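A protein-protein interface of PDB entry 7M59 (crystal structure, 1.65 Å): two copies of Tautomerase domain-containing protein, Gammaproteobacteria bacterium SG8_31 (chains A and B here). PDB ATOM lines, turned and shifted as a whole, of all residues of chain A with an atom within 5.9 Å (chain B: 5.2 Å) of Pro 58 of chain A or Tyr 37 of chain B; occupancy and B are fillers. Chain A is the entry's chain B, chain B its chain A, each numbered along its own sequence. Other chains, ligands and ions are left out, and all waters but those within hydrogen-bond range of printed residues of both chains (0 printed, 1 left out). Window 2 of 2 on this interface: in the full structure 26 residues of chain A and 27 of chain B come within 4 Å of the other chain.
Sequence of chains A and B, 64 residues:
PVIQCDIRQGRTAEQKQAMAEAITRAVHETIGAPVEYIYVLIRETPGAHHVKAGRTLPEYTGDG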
ATOM      1  N   ARG A   8     -13.398   6.933   0.534  1.00  0.00           N
ATOM      2  CA  ARG A   8     -14.215   6.000  -0.229  1.00  0.00           C
ATOM      3  C   ARG A   8     -14.306   4.656   0.500  1.00  0.00           C
ATOM      4  O   ARG A   8     -13.356   4.215   1.151  1.00  0.00           O
ATOM      5  CB  ARG A   8     -13.641   5.814  -1.637  1.00  0.00           C
ATOM      6  CG  ARG A   8     -13.968   6.959  -2.601  1.00  0.00           C
ATOM      7  CD  ARG A   8     -13.144   6.852  -3.894  1.00  0.00           C
ATOM      8  NE  ARG A   8     -11.726   6.990  -3.582  1.00  0.00           N
ATOM      9  CZ  ARG A   8     -10.743   6.282  -4.130  1.00  0.00           C
ATOM     10  NH1 ARG A   8     -10.998   5.372  -5.064  1.00  0.00           N
ATOM     11  NH2 ARG A   8      -9.498   6.486  -3.730  1.00  0.00           N
ATOM     12  N   GLY A  47     -17.435   5.925  -4.357  1.00  0.00           N
ATOM     13  CA  GLY A  47     -16.626   6.796  -5.196  1.00  0.00           C
ATOM     14  C   GLY A  47     -17.441   7.827  -5.950  1.00  0.00           C
ATOM     15  O   GLY A  47     -16.980   8.952  -6.162  1.00  0.00           O
ATOM     16  N   ALA A  48     -18.661   7.465  -6.358  1.00  0.00           N
ATOM     17  CA  ALA A  48     -19.520   8.369  -7.113  1.00  0.00           C
ATOM     18  C   ALA A  48     -19.930   9.584  -6.300  1.00  0.00           C
ATOM     19  O   ALA A  48     -20.406  10.569  -6.877  1.00  0.00           O
ATOM     20  CB  ALA A  48     -20.775   7.631  -7.591  1.00  0.00           C
ATOM     21  N   LYS A  52     -14.501  15.383  -8.085  1.00  0.00           N
ATOM     22  CA  LYS A  52     -13.336  16.255  -8.016  1.00  0.00           C
ATOM     23  C   LYS A  52     -13.068  16.803  -9.410  1.00  0.00           C
ATOM     24  O   LYS A  52     -12.914  16.031 -10.365  1.00  0.00           O
ATOM     25  CB  LYS A  52     -12.120  15.501  -7.476  1.00  0.00           C
ATOM     26  CG  LYS A  52     -10.832  16.335  -7.398  1.00  0.00           C
ATOM     27  CD  LYS A  52      -9.666  15.520  -6.839  1.00  0.00           C
ATOM     28  CE  LYS A  52      -9.177  14.456  -7.827  1.00  0.00           C
ATOM     29  NZ  LYS A  52      -8.557  14.997  -9.085  1.00  0.00           N
ATOM     30  N   THR A  56     -16.317  12.081 -11.266  1.00  0.00           N
ATOM     31  CA  THR A  56     -16.459  11.145 -10.157  1.00  0.00           C
ATOM     32  C   THR A  56     -15.179  10.338  -9.978  1.00  0.00           C
ATOM     33  O   THR A  56     -14.434  10.089 -10.932  1.00  0.00           O
ATOM     34  CB  THR A  56     -17.622  10.175 -10.361  1.00  0.00           C
ATOM     35  OG1 THR A  56     -17.377   9.365 -11.520  1.00  0.00           O
ATOM     36  CG2 THR A  56     -18.933  10.912 -10.514  1.00  0.00           C
ATOM     37  N   LEU A  57     -14.939   9.932  -8.764  1.00  0.00           N
ATOM     38  CA  LEU A  57     -13.812   9.061  -8.476  1.00  0.00           C
ATOM     39  C   LEU A  57     -14.222   7.597  -8.612  1.00  0.00           C
ATOM     40  O   LEU A  57     -15.383   7.243  -8.383  1.00  0.00           O
ATOM     41  CB  LEU A  57     -13.289   9.319  -7.059  1.00  0.00           C
ATOM     42  CG  LEU A  57     -12.737  10.711  -6.744  1.00  0.00           C
ATOM     43  CD1 LEU A  57     -11.962  10.706  -5.429  1.00  0.00           C
ATOM     44  CD2 LEU A  57     -11.865  11.238  -7.873  1.00  0.00           C
ATOM     45  N   PRO A  58     -13.295   6.726  -9.003  1.00  0.00           N
ATOM     46  CA  PRO A  58     -13.620   5.301  -9.103  1.00  0.00           C
ATOM     47  C   PRO A  58     -13.819   4.682  -7.732  1.00  0.00           C
ATOM     48  O   PRO A  58     -13.401   5.222  -6.705  1.00  0.00           O
ATOM     49  CB  PRO A  58     -12.392   4.707  -9.800  1.00  0.00           C
ATOM     50  CG  PRO A  58     -11.277   5.614  -9.396  1.00  0.00           C
ATOM     51  CD  PRO A  58     -11.878   7.000  -9.299  1.00  0.00           C
ATOM     52  N   GLU A  59     -14.487   3.530  -7.727  1.00  0.00           N
ATOM     53  CA  GLU A  59     -14.565   2.721  -6.520  1.00  0.00           C
ATOM     54  C   GLU A  59     -13.180   2.238  -6.119  1.00  0.00           C
ATOM     55  O   GLU A  59     -12.368   1.866  -6.972  1.00  0.00           O
ATOM     56  CB  GLU A  59     -15.475   1.513  -6.736  1.00  0.00           C
ATOM     57  CG  GLU A  59     -16.937   1.833  -6.710  1.00  0.00           C
ATOM     58  CD  GLU A  59     -17.389   2.282  -5.335  1.00  0.00           C
ATOM     59  OE1 GLU A  59     -17.216   1.531  -4.346  1.00  0.00           O
ATOM     60  OE2 GLU A  59     -17.905   3.399  -5.262  1.00  0.00           O
ATOM     61  N   TYR A  60     -12.916   2.232  -4.811  1.00  0.00           N
ATOM     62  CA  TYR A  60     -11.683   1.647  -4.294  1.00  0.00           C
ATOM     63  C   TYR A  60     -11.834   0.138  -4.135  1.00  0.00           C
ATOM     64  O   TYR A  60     -12.790  -0.337  -3.512  1.00  0.00           O
ATOM     65  CB  TYR A  60     -11.300   2.261  -2.942  1.00  0.00           C
ATOM     66  CG  TYR A  60     -10.113   1.552  -2.293  1.00  0.00           C
ATOM     67  CD1 TYR A  60     -10.301   0.468  -1.431  1.00  0.00           C
ATOM     68  CD2 TYR A  60      -8.811   1.959  -2.560  1.00  0.00           C
ATOM     69  CE1 TYR A  60      -9.224  -0.181  -0.853  1.00  0.00           C
ATOM     70  CE2 TYR A  60      -7.725   1.314  -1.985  1.00  0.00           C
ATOM     71  CZ  TYR A  60      -7.940   0.247  -1.136  1.00  0.00           C
ATOM     72  OH  TYR A  60      -6.862  -0.394  -0.571  1.00  0.00           O
ATOM     73  N   PRO B   1      -9.898  11.700  -1.049  1.00  0.00           N
ATOM     74  CA  PRO B   1     -10.622  11.890   0.220  1.00  0.00           C
ATOM     75  C   PRO B   1     -10.490  13.313   0.720  1.00  0.00           C
ATOM     76  O   PRO B   1      -9.566  14.018   0.313  1.00  0.00           O
ATOM     77  CB  PRO B   1      -9.920  10.925   1.181  1.00  0.00           C
ATOM     78  CG  PRO B   1      -8.523  10.808   0.612  1.00  0.00           C
ATOM     79  CD  PRO B   1      -8.725  10.819  -0.879  1.00  0.00           C
ATOM     80  N   ALA B  33      -5.111   5.820  -0.900  1.00  0.00           N
ATOM     81  CA  ALA B  33      -5.640   6.929  -1.674  1.00  0.00           C
ATOM     82  C   ALA B  33      -4.500   7.571  -2.453  1.00  0.00           C
ATOM     83  O   ALA B  33      -3.462   7.898  -1.863  1.00  0.00           O
ATOM     84  CB  ALA B  33      -6.297   7.959  -0.754  1.00  0.00           C
ATOM     85  N   PRO B  34      -4.635   7.742  -3.766  1.00  0.00           N
ATOM     86  CA  PRO B  34      -3.599   8.469  -4.504  1.00  0.00           C
ATOM     87  C   PRO B  34      -3.464   9.879  -3.965  1.00  0.00           C
ATOM     88  O   PRO B  34      -4.449  10.513  -3.585  1.00  0.00           O
ATOM     89  CB  PRO B  34      -4.100   8.458  -5.954  1.00  0.00           C
ATOM     90  CG  PRO B  34      -5.399   7.775  -5.959  1.00  0.00           C
ATOM     91  CD  PRO B  34      -5.630   7.111  -4.647  1.00  0.00           C
ATOM     92  N   VAL B  35      -2.222  10.360  -3.921  1.00  0.00           N
ATOM     93  CA  VAL B  35      -1.975  11.712  -3.427  1.00  0.00           C
ATOM     94  C   VAL B  35      -2.822  12.719  -4.194  1.00  0.00           C
ATOM     95  O   VAL B  35      -3.338  13.684  -3.618  1.00  0.00           O
ATOM     96  CB  VAL B  35      -0.474  12.039  -3.511  1.00  0.00           C
ATOM     97  CG1 VAL B  35      -0.220  13.504  -3.185  1.00  0.00           C
ATOM     98  CG2 VAL B  35       0.305  11.129  -2.577  1.00  0.00           C
ATOM     99  N   GLU B  36      -3.021  12.483  -5.493  1.00  0.00           N
ATOM    100  CA  GLU B  36      -3.804  13.398  -6.320  1.00  0.00           C
ATOM    101  C   GLU B  36      -5.246  13.544  -5.824  1.00  0.00           C
ATOM    102  O   GLU B  36      -5.866  14.591  -6.057  1.00  0.00           O
ATOM    103  CB  GLU B  36      -3.780  12.923  -7.780  1.00  0.00           C
ATOM    104  CG  GLU B  36      -4.952  13.409  -8.625  1.00  0.00           C
ATOM    105  CD  GLU B  36      -4.992  12.805 -10.012  1.00  0.00           C
ATOM    106  OE1 GLU B  36      -3.932  12.353 -10.504  1.00  0.00           O
ATOM    107  OE2 GLU B  36      -6.097  12.781 -10.604  1.00  0.00           O
ATOM    108  N   TYR B  37      -5.787  12.534  -5.137  1.00  0.00           N
ATOM    109  CA  TYR B  37      -7.164  12.570  -4.646  1.00  0.00           C
ATOM    110  C   TYR B  37      -7.303  13.216  -3.272  1.00  0.00           C
ATOM    111  O   TYR B  37      -8.436  13.406  -2.811  1.00  0.00           O
ATOM    112  CB  TYR B  37      -7.754  11.157  -4.536  1.00  0.00           C
ATOM    113  CG  TYR B  37      -8.024  10.417  -5.830  1.00  0.00           C
ATOM    114  CD1 TYR B  37      -8.616   9.164  -5.801  1.00  0.00           C
ATOM    115  CD2 TYR B  37      -7.686  10.961  -7.064  1.00  0.00           C
ATOM    116  CE1 TYR B  37      -8.875   8.460  -6.962  1.00  0.00           C
ATOM    117  CE2 TYR B  37      -7.937  10.260  -8.244  1.00  0.00           C
ATOM    118  CZ  TYR B  37      -8.529   9.009  -8.178  1.00  0.00           C
ATOM    119  OH  TYR B  37      -8.793   8.301  -9.331  1.00  0.00           O
ATOM    120  N   ILE B  38      -6.208  13.532  -2.594  1.00  0.00           N
ATOM    121  CA  ILE B  38      -6.273  13.940  -1.193  1.00  0.00           C
ATOM    122  C   ILE B  38      -6.426  15.455  -1.110  1.00  0.00           C
ATOM    123  O   ILE B  38      -5.722  16.208  -1.796  1.00  0.00           O
ATOM    124  CB  ILE B  38      -5.033  13.465  -0.422  1.00  0.00           C
ATOM    125  CG1 ILE B  38      -4.974  11.933  -0.410  1.00  0.00           C
ATOM    126  CG2 ILE B  38      -5.050  14.014   0.995  1.00  0.00           C
ATOM    127  CD1 ILE B  38      -3.696  11.375   0.179  1.00  0.00           C
ATOM    128  N   TYR B  39      -7.352  15.909  -0.266  1.00  0.00           N
ATOM    129  CA  TYR B  39      -7.577  17.331  -0.034  1.00  0.00           C
ATOM    130  C   TYR B  39      -7.645  17.516   1.477  1.00  0.00           C
ATOM    131  O   TYR B  39      -8.550  16.981   2.127  1.00  0.00           O
ATOM    132  CB  TYR B  39      -8.863  17.788  -0.726  1.00  0.00           C
ATOM    133  CG  TYR B  39      -9.088  19.280  -0.922  1.00  0.00           C
ATOM    134  CD1 TYR B  39      -9.599  19.756  -2.125  1.00  0.00           C
ATOM    135  CD2 TYR B  39      -8.868  20.204   0.107  1.00  0.00           C
ATOM    136  CE1 TYR B  39      -9.855  21.106  -2.317  1.00  0.00           C
ATOM    137  CE2 TYR B  39      -9.119  21.564  -0.083  1.00  0.00           C
ATOM    138  CZ  TYR B  39      -9.616  22.000  -1.299  1.00  0.00           C
ATOM    139  OH  TYR B  39      -9.891  23.330  -1.508  1.00  0.00           O
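Of the printed residues of chain B, Arg 8 of chain A touches Tyr 37 (3.5 Å). Of the printed residues of chain B, Leu 57 of chain A touches Tyr 37. Of chain B, only Tyr 37 (3.3 Å) comes within 4 Å of Pro 58 of chain A. Printed residues of chain A within 4 Å of Glu 36 of chain B: Lys 52. Tyr 37 of chain B touches just these residues of chain A: Arg 8, Lys 52, Leu 57 and Pro 58. The nearest printed residue of chain B that does not touch Pro 58 of chain A is Pro 34 of chain B (7.1 Å).
Among the printed residues, pairs that only touch across the chains: Pro 58 of chain A with Tyr 37 of chain B (3.3 Å), Arg 8 of chain A with Tyr 37 of chain B (3.5 Å), Leu 57 of chain A with Tyr 37 of chain B (3.7 Å) and Lys 52 of chain A with Tyr 37 of chain B (3.9 Å).
No position is printed for both chains. Of the 5 pairs that touch across the chains among the printed residues, none has its exchanged pair printed and touching as well.
The guanidinium group (NH1) of Arg 8 of chain A is in hydrogen-bond range of the backbone carbonyl oxygen (O) of Pro 58 of chain A (2.9 Å). N of Leu 57 of chain A sits at hydrogen-bond distance from O of Gly 47 of chain A, 3.4 Å away.
OE2 of Glu 36 of chain B lies within salt-bridge range of NZ of Lys 52 of chain A.
Hydrophobic or aromatic side chains of chain A within 4 Å of the printed part of chain B: Leu 57 and Pro 58. Among the printed residues, 5 pairs touch across the chains. Among the printed residues, Asp or Glu carboxylates within 4 Å of a Lys or Arg side-chain nitrogen of the other chain: Lys 52 of chain A with Glu 36 of chain B.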
